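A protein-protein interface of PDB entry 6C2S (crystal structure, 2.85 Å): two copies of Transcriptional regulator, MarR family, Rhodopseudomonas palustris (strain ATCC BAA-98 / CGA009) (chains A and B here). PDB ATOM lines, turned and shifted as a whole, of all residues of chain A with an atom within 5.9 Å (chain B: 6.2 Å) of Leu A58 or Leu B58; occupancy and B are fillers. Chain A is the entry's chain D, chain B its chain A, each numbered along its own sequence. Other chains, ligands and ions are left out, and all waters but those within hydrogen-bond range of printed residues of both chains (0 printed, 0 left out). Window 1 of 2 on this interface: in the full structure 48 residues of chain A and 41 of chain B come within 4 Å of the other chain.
The side-chain amide oxygen (OE1) of Gln B62 sits close to the side-chain amide oxygen (OE1) of Gln A62 (3.0 Å).
Leu A58 touches five residues of chain B.
Of the printed residues of chain A, Leu B58 touches Leu A58 (3.7 Å), Val A65 (3.8 Å) and Leu A179 (3.7 Å).
Of the printed residues of chain B, Ile A182 touches Val B65 and Leu B175.
Printed residues of chain B within 4 Å of Leu A175: Leu B54, Leu B175, Leu B179 and Ile B182.
Leu B63 touches none of the printed residues of chain A.
Leu A63 touches none of the printed residues of chain B.
The nearest residue of chain B that does not touch Leu A58 is Leu B175 (5.5 Å).
Of the 16 printed residues of chain B, 12 touch a printed residue of chain A.
Of the 16 printed residues of chain A, 11 touch a printed residue of chain B.
Printed residues of chain A that touch a printed residue of chain B: Gly A55, Ala A57, Leu A58, Lys A59, Ala A61, Gln A62, Val A65, Phe A66, Leu A175, Leu A179 and Ile A182.
Hydrophobic or aromatic side chains of chain A that line the printed part of chain B: Leu A58, Ala A61, Val A65, Phe A66, Leu A175, Leu A179 and Ile A182.
Along chain A the printed residues that touch a printed residue of chain B span positions 55 to 182.
Among the printed residues, no Asp or Glu carboxylate lies within 4 Å of a Lys or Arg side-chain nitrogen of the other chain.
Ala A57 touches Leu B179, and with the chains exchanged Leu A179 touches Ala B57.
Leu A58 touches Ala B61, but with the chains exchanged Ala A61 does not touch Leu B58 (4.1 Å).
Leu A58 touches Val B65, and with the chains exchanged Val A65 touches Leu B58.
Val A65 touches Ile B182, and with the chains exchanged Ile A182 touches Val B65.
16 positions are printed for both chains.
Gly A55 touches Phe B66 (O to CE1, 3.5 Å).
Leu B179 touches Ala A57 (CB to O, 3.6 Å).
Leu A58 touches Leu B58 (CD1 to CD2, 3.7 Å).
Val B65 touches Leu A58.
CZ of Phe A66 touches CE of Lys B59, 3.3 Å away.
CD1 of Leu A175 touches CD2 of Leu B179, 3.9 Å away.
Ile B182 touches Leu A175 (CD1 to CD2, 3.8 Å).
Leu A179 touches Ala B57.
Leu A179 touches Ala B61.
Ile A182 touches Val B65.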
ATOM      1  N   LEU A  53      26.182  10.682 -16.720  1.00  0.00           N
ATOM      2  CA  LEU A  53      24.918  10.238 -17.300  1.00  0.00           C
ATOM      3  C   LEU A  53      25.017   8.737 -17.513  1.00  0.00           C
ATOM      4  O   LEU A  53      25.841   8.263 -18.303  1.00  0.00           O
ATOM      5  CB  LEU A  53      24.635  10.965 -18.613  1.00  0.00           C
ATOM      6  CG  LEU A  53      23.221  11.125 -19.197  1.00  0.00           C
ATOM      7  CD1 LEU A  53      22.634   9.829 -19.736  1.00  0.00           C
ATOM      8  CD2 LEU A  53      22.270  11.752 -18.175  1.00  0.00           C
ATOM      9  N   LEU A  54      24.180   7.986 -16.799  1.00  0.00           N
ATOM     10  CA  LEU A  54      24.271   6.536 -16.858  1.00  0.00           C
ATOM     11  C   LEU A  54      23.783   6.042 -18.207  1.00  0.00           C
ATOM     12  O   LEU A  54      24.350   5.104 -18.774  1.00  0.00           O
ATOM     13  CB  LEU A  54      23.471   5.925 -15.706  1.00  0.00           C
ATOM     14  CG  LEU A  54      23.657   4.476 -15.230  1.00  0.00           C
ATOM     15  CD1 LEU A  54      23.336   3.419 -16.285  1.00  0.00           C
ATOM     16  CD2 LEU A  54      25.065   4.294 -14.686  1.00  0.00           C
ATOM     17  N   GLY A  55      22.723   6.661 -18.731  1.00  0.00           N
ATOM     18  CA  GLY A  55      22.265   6.322 -20.067  1.00  0.00           C
ATOM     19  C   GLY A  55      23.388   6.320 -21.083  1.00  0.00           C
ATOM     20  O   GLY A  55      23.558   5.356 -21.834  1.00  0.00           O
ATOM     21  N   TYR A  56      24.178   7.398 -21.106  1.00  0.00           N
ATOM     22  CA  TYR A  56      25.261   7.539 -22.079  1.00  0.00           C
ATOM     23  C   TYR A  56      26.307   6.441 -21.909  1.00  0.00           C
ATOM     24  O   TYR A  56      26.789   5.863 -22.895  1.00  0.00           O
ATOM     25  CB  TYR A  56      25.892   8.932 -21.956  1.00  0.00           C
ATOM     26  CG  TYR A  56      27.024   9.229 -22.933  1.00  0.00           C
ATOM     27  CD1 TYR A  56      28.341   8.879 -22.647  1.00  0.00           C
ATOM     28  CD2 TYR A  56      26.771   9.873 -24.141  1.00  0.00           C
ATOM     29  CE1 TYR A  56      29.365   9.153 -23.535  1.00  0.00           C
ATOM     30  CE2 TYR A  56      27.798  10.156 -25.042  1.00  0.00           C
ATOM     31  CZ  TYR A  56      29.091   9.797 -24.732  1.00  0.00           C
ATOM     32  OH  TYR A  56      30.113  10.073 -25.624  1.00  0.00           O
ATOM     33  N   ALA A  57      26.706   6.166 -20.665  1.00  0.00           N
ATOM     34  CA  ALA A  57      27.695   5.121 -20.438  1.00  0.00           C
ATOM     35  C   ALA A  57      27.148   3.764 -20.851  1.00  0.00           C
ATOM     36  O   ALA A  57      27.889   2.898 -21.329  1.00  0.00           O
ATOM     37  CB  ALA A  57      28.132   5.112 -18.974  1.00  0.00           C
ATOM     38  N   LEU A  58      25.851   3.557 -20.641  1.00  0.00           N
ATOM     39  CA  LEU A  58      25.199   2.311 -21.029  1.00  0.00           C
ATOM     40  C   LEU A  58      25.220   2.104 -22.541  1.00  0.00           C
ATOM     41  O   LEU A  58      25.518   1.008 -23.027  1.00  0.00           O
ATOM     42  CB  LEU A  58      23.777   2.304 -20.472  1.00  0.00           C
ATOM     43  CG  LEU A  58      23.264   0.955 -20.021  1.00  0.00           C
ATOM     44  CD1 LEU A  58      24.389   0.121 -19.467  1.00  0.00           C
ATOM     45  CD2 LEU A  58      22.280   1.233 -18.939  1.00  0.00           C
ATOM     46  N   LYS A  59      24.865   3.137 -23.305  1.00  0.00           N
ATOM     47  CA  LYS A  59      24.860   2.993 -24.758  1.00  0.00           C
ATOM     48  C   LYS A  59      26.271   2.797 -25.308  1.00  0.00           C
ATOM     49  O   LYS A  59      26.502   1.886 -26.113  1.00  0.00           O
ATOM     50  CB  LYS A  59      24.193   4.198 -25.424  1.00  0.00           C
ATOM     51  CG  LYS A  59      24.150   4.102 -26.956  1.00  0.00           C
ATOM     52  CD  LYS A  59      23.212   2.963 -27.381  1.00  0.00           C
ATOM     53  CE  LYS A  59      23.002   2.827 -28.895  1.00  0.00           C
ATOM     54  NZ  LYS A  59      21.818   1.933 -29.185  1.00  0.00           N
ATOM     55  N   ARG A  60      27.240   3.613 -24.864  1.00  0.00           N
ATOM     56  CA  ARG A  60      28.571   3.510 -25.464  1.00  0.00           C
ATOM     57  C   ARG A  60      29.264   2.225 -25.035  1.00  0.00           C
ATOM     58  O   ARG A  60      30.050   1.650 -25.796  1.00  0.00           O
ATOM     59  CB  ARG A  60      29.448   4.720 -25.118  1.00  0.00           C
ATOM     60  CG  ARG A  60      28.879   6.087 -25.550  1.00  0.00           C
ATOM     61  CD  ARG A  60      29.061   6.441 -27.037  1.00  0.00           C
ATOM     62  NE  ARG A  60      30.375   6.944 -27.444  1.00  0.00           N
ATOM     63  CZ  ARG A  60      30.798   6.926 -28.710  1.00  0.00           C
ATOM     64  NH1 ARG A  60      30.000   6.452 -29.665  1.00  0.00           N
ATOM     65  NH2 ARG A  60      32.004   7.392 -29.034  1.00  0.00           N
ATOM     66  N   ALA A  61      28.965   1.743 -23.832  1.00  0.00           N
ATOM     67  CA  ALA A  61      29.441   0.426 -23.432  1.00  0.00           C
ATOM     68  C   ALA A  61      28.845  -0.667 -24.308  1.00  0.00           C
ATOM     69  O   ALA A  61      29.524  -1.649 -24.636  1.00  0.00           O
ATOM     70  CB  ALA A  61      29.124   0.174 -21.958  1.00  0.00           C
ATOM     71  N   GLN A  62      27.565  -0.542 -24.662  1.00  0.00           N
ATOM     72  CA  GLN A  62      26.933  -1.569 -25.477  1.00  0.00           C
ATOM     73  C   GLN A  62      27.548  -1.667 -26.872  1.00  0.00           C
ATOM     74  O   GLN A  62      27.742  -2.768 -27.395  1.00  0.00           O
ATOM     75  CB  GLN A  62      25.432  -1.308 -25.574  1.00  0.00           C
ATOM     76  CG  GLN A  62      24.732  -2.274 -26.518  1.00  0.00           C
ATOM     77  CD  GLN A  62      23.699  -1.592 -27.397  1.00  0.00           C
ATOM     78  OE1 GLN A  62      22.767  -0.961 -26.895  1.00  0.00           O
ATOM     79  NE2 GLN A  62      23.911  -1.644 -28.718  1.00  0.00           N
ATOM     80  N   LEU A  63      27.857  -0.532 -27.489  1.00  0.00           N
ATOM     81  CA  LEU A  63      28.319  -0.550 -28.872  1.00  0.00           C
ATOM     82  C   LEU A  63      29.706  -1.176 -29.008  1.00  0.00           C
ATOM     83  O   LEU A  63      29.967  -1.892 -29.966  1.00  0.00           O
ATOM     84  CB  LEU A  63      28.277   0.863 -29.434  1.00  0.00           C
ATOM     85  CG  LEU A  63      26.832   1.265 -29.747  1.00  0.00           C
ATOM     86  CD1 LEU A  63      26.600   2.742 -29.448  1.00  0.00           C
ATOM     87  CD2 LEU A  63      26.577   0.940 -31.196  1.00  0.00           C
ATOM     88  N   VAL A  65      30.826  -3.518 -27.118  1.00  0.00           N
ATOM     89  CA  VAL A  65      30.554  -4.939 -26.924  1.00  0.00           C
ATOM     90  C   VAL A  65      29.905  -5.542 -28.164  1.00  0.00           C
ATOM     91  O   VAL A  65      30.283  -6.628 -28.613  1.00  0.00           O
ATOM     92  CB  VAL A  65      29.691  -5.153 -25.673  1.00  0.00           C
ATOM     93  CG1 VAL A  65      29.351  -6.626 -25.541  1.00  0.00           C
ATOM     94  CG2 VAL A  65      30.423  -4.632 -24.441  1.00  0.00           C
ATOM     95  N   PHE A  66      28.906  -4.856 -28.725  1.00  0.00           N
ATOM     96  CA  PHE A  66      28.268  -5.356 -29.937  1.00  0.00           C
ATOM     97  C   PHE A  66      29.257  -5.411 -31.092  1.00  0.00           C
ATOM     98  O   PHE A  66      29.294  -6.397 -31.843  1.00  0.00           O
ATOM     99  CB  PHE A  66      27.059  -4.484 -30.279  1.00  0.00           C
ATOM    100  CG  PHE A  66      25.744  -5.054 -29.786  1.00  0.00           C
ATOM    101  CD1 PHE A  66      25.605  -5.502 -28.469  1.00  0.00           C
ATOM    102  CD2 PHE A  66      24.644  -5.131 -30.629  1.00  0.00           C
ATOM    103  CE1 PHE A  66      24.410  -6.031 -28.010  1.00  0.00           C
ATOM    104  CE2 PHE A  66      23.435  -5.653 -30.171  1.00  0.00           C
ATOM    105  CZ  PHE A  66      23.322  -6.104 -28.858  1.00  0.00           C
ATOM    106  N   LEU A 175      28.396  -6.791 -12.571  1.00  0.00           N
ATOM    107  CA  LEU A 175      27.896  -6.019 -13.706  1.00  0.00           C
ATOM    108  C   LEU A 175      26.707  -6.718 -14.365  1.00  0.00           C
ATOM    109  O   LEU A 175      25.653  -6.108 -14.573  1.00  0.00           O
ATOM    110  CB  LEU A 175      29.029  -5.780 -14.712  1.00  0.00           C
ATOM    111  CG  LEU A 175      28.684  -5.212 -16.093  1.00  0.00           C
ATOM    112  CD1 LEU A 175      28.246  -3.777 -15.985  1.00  0.00           C
ATOM    113  CD2 LEU A 175      29.833  -5.371 -17.068  1.00  0.00           C
ATOM    114  N   LEU A 179      22.892  -5.180 -14.541  1.00  0.00           N
ATOM    115  CA  LEU A 179      22.214  -4.963 -15.816  1.00  0.00           C
ATOM    116  C   LEU A 179      20.956  -5.812 -15.908  1.00  0.00           C
ATOM    117  O   LEU A 179      19.967  -5.404 -16.529  1.00  0.00           O
ATOM    118  CB  LEU A 179      23.148  -5.262 -16.986  1.00  0.00           C
ATOM    119  CG  LEU A 179      24.440  -4.460 -17.119  1.00  0.00           C
ATOM    120  CD1 LEU A 179      25.360  -5.132 -18.127  1.00  0.00           C
ATOM    121  CD2 LEU A 179      24.142  -3.025 -17.542  1.00  0.00           C
ATOM    122  N   ILE A 182      18.306  -4.026 -13.780  1.00  0.00           N
ATOM    123  CA  ILE A 182      17.767  -2.844 -14.459  1.00  0.00           C
ATOM    124  C   ILE A 182      16.667  -3.218 -15.451  1.00  0.00           C
ATOM    125  O   ILE A 182      15.652  -2.520 -15.563  1.00  0.00           O
ATOM    126  CB  ILE A 182      18.896  -2.034 -15.134  1.00  0.00           C
ATOM    127  CG1 ILE A 182      19.843  -1.437 -14.090  1.00  0.00           C
ATOM    128  CG2 ILE A 182      18.332  -0.913 -16.019  1.00  0.00           C
ATOM    129  CD1 ILE A 182      21.092  -0.834 -14.690  1.00  0.00           C
ATOM    130  N   LEU B  53      25.013 -13.901 -21.377  1.00  0.00           N
ATOM    131  CA  LEU B  53      25.704 -13.075 -22.364  1.00  0.00           C
ATOM    132  C   LEU B  53      25.652 -11.619 -21.942  1.00  0.00           C
ATOM    133  O   LEU B  53      24.560 -11.052 -21.780  1.00  0.00           O
ATOM    134  CB  LEU B  53      25.129 -13.217 -23.763  1.00  0.00           C
ATOM    135  CG  LEU B  53      25.264 -14.580 -24.397  1.00  0.00           C
ATOM    136  CD1 LEU B  53      25.252 -14.284 -25.870  1.00  0.00           C
ATOM    137  CD2 LEU B  53      26.486 -15.421 -23.912  1.00  0.00           C
ATOM    138  N   LEU B  54      26.826 -11.012 -21.750  1.00  0.00           N
ATOM    139  CA  LEU B  54      26.846  -9.659 -21.226  1.00  0.00           C
ATOM    140  C   LEU B  54      26.348  -8.653 -22.260  1.00  0.00           C
ATOM    141  O   LEU B  54      25.636  -7.704 -21.908  1.00  0.00           O
ATOM    142  CB  LEU B  54      28.238  -9.307 -20.744  1.00  0.00           C
ATOM    143  CG  LEU B  54      28.214  -8.016 -19.929  1.00  0.00           C
ATOM    144  CD1 LEU B  54      27.325  -8.163 -18.696  1.00  0.00           C
ATOM    145  CD2 LEU B  54      29.616  -7.682 -19.534  1.00  0.00           C
ATOM    146  N   GLY B  55      26.715  -8.828 -23.540  1.00  0.00           N
ATOM    147  CA  GLY B  55      26.173  -7.962 -24.580  1.00  0.00           C
ATOM    148  C   GLY B  55      24.662  -7.866 -24.525  1.00  0.00           C
ATOM    149  O   GLY B  55      24.087  -6.772 -24.548  1.00  0.00           O
ATOM    150  N   TYR B  56      23.997  -9.022 -24.452  1.00  0.00           N
ATOM    151  CA  TYR B  56      22.540  -9.047 -24.412  1.00  0.00           C
ATOM    152  C   TYR B  56      22.004  -8.270 -23.218  1.00  0.00           C
ATOM    153  O   TYR B  56      21.053  -7.491 -23.357  1.00  0.00           O
ATOM    154  CB  TYR B  56      22.039 -10.487 -24.376  1.00  0.00           C
ATOM    155  CG  TYR B  56      20.532 -10.593 -24.296  1.00  0.00           C
ATOM    156  CD1 TYR B  56      19.750 -10.510 -25.445  1.00  0.00           C
ATOM    157  CD2 TYR B  56      19.887 -10.771 -23.072  1.00  0.00           C
ATOM    158  CE1 TYR B  56      18.368 -10.604 -25.384  1.00  0.00           C
ATOM    159  CE2 TYR B  56      18.510 -10.861 -22.997  1.00  0.00           C
ATOM    160  CZ  TYR B  56      17.749 -10.780 -24.159  1.00  0.00           C
ATOM    161  OH  TYR B  56      16.366 -10.872 -24.103  1.00  0.00           O
ATOM    162  N   ALA B  57      22.602  -8.457 -22.035  1.00  0.00           N
ATOM    163  CA  ALA B  57      22.101  -7.764 -20.851  1.00  0.00           C
ATOM    164  C   ALA B  57      22.212  -6.264 -21.019  1.00  0.00           C
ATOM    165  O   ALA B  57      21.294  -5.518 -20.647  1.00  0.00           O
ATOM    166  CB  ALA B  57      22.863  -8.215 -19.607  1.00  0.00           C
ATOM    167  N   LEU B  58      23.310  -5.816 -21.640  1.00  0.00           N
ATOM    168  CA  LEU B  58      23.512  -4.408 -21.949  1.00  0.00           C
ATOM    169  C   LEU B  58      22.435  -3.885 -22.879  1.00  0.00           C
ATOM    170  O   LEU B  58      21.949  -2.761 -22.704  1.00  0.00           O
ATOM    171  CB  LEU B  58      24.883  -4.193 -22.576  1.00  0.00           C
ATOM    172  CG  LEU B  58      26.059  -4.059 -21.631  1.00  0.00           C
ATOM    173  CD1 LEU B  58      27.273  -4.546 -22.367  1.00  0.00           C
ATOM    174  CD2 LEU B  58      26.218  -2.623 -21.175  1.00  0.00           C
ATOM    175  N   LYS B  59      22.064  -4.571 -23.930  1.00  0.00           N
ATOM    176  CA  LYS B  59      21.081  -3.898 -24.746  1.00  0.00           C
ATOM    177  C   LYS B  59      19.776  -3.717 -24.042  1.00  0.00           C
ATOM    178  O   LYS B  59      19.260  -2.631 -24.000  1.00  0.00           O
ATOM    179  CB  LYS B  59      20.893  -4.517 -26.126  1.00  0.00           C
ATOM    180  CG  LYS B  59      20.439  -5.954 -26.122  1.00  0.00           C
ATOM    181  CD  LYS B  59      20.200  -6.467 -27.534  1.00  0.00           C
ATOM    182  CE  LYS B  59      20.790  -7.856 -27.727  1.00  0.00           C
ATOM    183  NZ  LYS B  59      20.606  -8.371 -29.105  1.00  0.00           N
ATOM    184  N   ARG B  60      19.250  -4.758 -23.432  1.00  0.00           N
ATOM    185  CA  ARG B  60      17.945  -4.588 -22.805  1.00  0.00           C
ATOM    186  C   ARG B  60      18.051  -3.674 -21.587  1.00  0.00           C
ATOM    187  O   ARG B  60      17.072  -3.052 -21.183  1.00  0.00           O
ATOM    188  CB  ARG B  60      17.319  -5.939 -22.444  1.00  0.00           C
ATOM    189  CG  ARG B  60      17.610  -7.082 -23.421  1.00  0.00           C
ATOM    190  CD  ARG B  60      16.684  -7.107 -24.678  1.00  0.00           C
ATOM    191  NE  ARG B  60      15.275  -6.782 -24.434  1.00  0.00           N
ATOM    192  CZ  ARG B  60      14.293  -7.648 -24.183  1.00  0.00           C
ATOM    193  NH1 ARG B  60      14.515  -8.958 -24.131  1.00  0.00           N
ATOM    194  NH2 ARG B  60      13.061  -7.185 -23.991  1.00  0.00           N
ATOM    195  N   ALA B  61      19.216  -3.638 -20.948  1.00  0.00           N
ATOM    196  CA  ALA B  61      19.469  -2.619 -19.928  1.00  0.00           C
ATOM    197  C   ALA B  61      19.537  -1.223 -20.535  1.00  0.00           C
ATOM    198  O   ALA B  61      19.097  -0.251 -19.915  1.00  0.00           O
ATOM    199  CB  ALA B  61      20.754  -2.933 -19.165  1.00  0.00           C
ATOM    200  N   GLN B  62      20.170  -1.081 -21.703  1.00  0.00           N
ATOM    201  CA  GLN B  62      20.234   0.232 -22.333  1.00  0.00           C
ATOM    202  C   GLN B  62      18.852   0.697 -22.786  1.00  0.00           C
ATOM    203  O   GLN B  62      18.476   1.856 -22.557  1.00  0.00           O
ATOM    204  CB  GLN B  62      21.195   0.207 -23.518  1.00  0.00           C
ATOM    205  CG  GLN B  62      21.423   1.562 -24.151  1.00  0.00           C
ATOM    206  CD  GLN B  62      20.650   1.689 -25.408  1.00  0.00           C
ATOM    207  OE1 GLN B  62      20.411   0.706 -26.099  1.00  0.00           O
ATOM    208  NE2 GLN B  62      20.203   2.896 -25.702  1.00  0.00           N
ATOM    209  N   LEU B  63      18.055  -0.209 -23.365  1.00  0.00           N
ATOM    210  CA  LEU B  63      16.791   0.210 -23.969  1.00  0.00           C
ATOM    211  C   LEU B  63      15.781   0.680 -22.925  1.00  0.00           C
ATOM    212  O   LEU B  63      15.068   1.666 -23.155  1.00  0.00           O
ATOM    213  CB  LEU B  63      16.198  -0.909 -24.820  1.00  0.00           C
ATOM    214  CG  LEU B  63      16.857  -1.215 -26.173  1.00  0.00           C
ATOM    215  CD1 LEU B  63      16.198  -2.415 -26.821  1.00  0.00           C
ATOM    216  CD2 LEU B  63      16.790  -0.012 -27.069  1.00  0.00           C
ATOM    217  N   VAL B  65      16.572   1.956 -19.941  1.00  0.00           N
ATOM    218  CA  VAL B  65      17.062   3.218 -19.391  1.00  0.00           C
ATOM    219  C   VAL B  65      16.761   4.350 -20.357  1.00  0.00           C
ATOM    220  O   VAL B  65      16.285   5.412 -19.949  1.00  0.00           O
ATOM    221  CB  VAL B  65      18.562   3.156 -19.056  1.00  0.00           C
ATOM    222  CG1 VAL B  65      18.984   4.504 -18.536  1.00  0.00           C
ATOM    223  CG2 VAL B  65      18.832   2.120 -18.012  1.00  0.00           C
ATOM    224  N   PHE B  66      17.002   4.136 -21.655  1.00  0.00           N
ATOM    225  CA  PHE B  66      16.664   5.177 -22.624  1.00  0.00           C
ATOM    226  C   PHE B  66      15.166   5.458 -22.632  1.00  0.00           C
ATOM    227  O   PHE B  66      14.745   6.623 -22.563  1.00  0.00           O
ATOM    228  CB  PHE B  66      17.150   4.784 -24.021  1.00  0.00           C
ATOM    229  CG  PHE B  66      18.500   5.376 -24.387  1.00  0.00           C
ATOM    230  CD1 PHE B  66      19.447   5.666 -23.393  1.00  0.00           C
ATOM    231  CD2 PHE B  66      18.829   5.643 -25.713  1.00  0.00           C
ATOM    232  CE1 PHE B  66      20.687   6.202 -23.697  1.00  0.00           C
ATOM    233  CE2 PHE B  66      20.085   6.181 -26.038  1.00  0.00           C
ATOM    234  CZ  PHE B  66      21.012   6.463 -25.020  1.00  0.00           C
ATOM    235  N   LEU B 175      28.950   0.379 -11.356  1.00  0.00           N
ATOM    236  CA  LEU B 175      28.409   0.090 -12.678  1.00  0.00           C
ATOM    237  C   LEU B 175      28.883   1.136 -13.697  1.00  0.00           C
ATOM    238  O   LEU B 175      29.366   0.813 -14.788  1.00  0.00           O
ATOM    239  CB  LEU B 175      26.886   0.045 -12.595  1.00  0.00           C
ATOM    240  CG  LEU B 175      26.225  -0.009 -13.961  1.00  0.00           C
ATOM    241  CD1 LEU B 175      26.531  -1.368 -14.447  1.00  0.00           C
ATOM    242  CD2 LEU B 175      24.723   0.222 -13.928  1.00  0.00           C
ATOM    243  N   LEU B 179      31.181   0.369 -17.096  1.00  0.00           N
ATOM    244  CA  LEU B 179      30.758   0.696 -18.452  1.00  0.00           C
ATOM    245  C   LEU B 179      31.729   1.680 -19.081  1.00  0.00           C
ATOM    246  O   LEU B 179      31.990   1.629 -20.291  1.00  0.00           O
ATOM    247  CB  LEU B 179      29.350   1.284 -18.423  1.00  0.00           C
ATOM    248  CG  LEU B 179      28.275   0.437 -17.745  1.00  0.00           C
ATOM    249  CD1 LEU B 179      27.070   1.318 -17.489  1.00  0.00           C
ATOM    250  CD2 LEU B 179      27.904  -0.798 -18.550  1.00  0.00           C
ATOM    251  N   ILE B 182      34.669  -0.412 -20.021  1.00  0.00           N
ATOM    252  CA  ILE B 182      34.414  -1.249 -21.189  1.00  0.00           C
ATOM    253  C   ILE B 182      34.630  -0.458 -22.464  1.00  0.00           C
ATOM    254  O   ILE B 182      35.267  -0.941 -23.407  1.00  0.00           O
ATOM    255  CB  ILE B 182      33.003  -1.857 -21.144  1.00  0.00           C
ATOM    256  CG1 ILE B 182      32.882  -2.835 -19.990  1.00  0.00           C
ATOM    257  CG2 ILE B 182      32.688  -2.547 -22.454  1.00  0.00           C
ATOM    258  CD1 ILE B 182      31.471  -3.279 -19.746  1.00  0.00           C
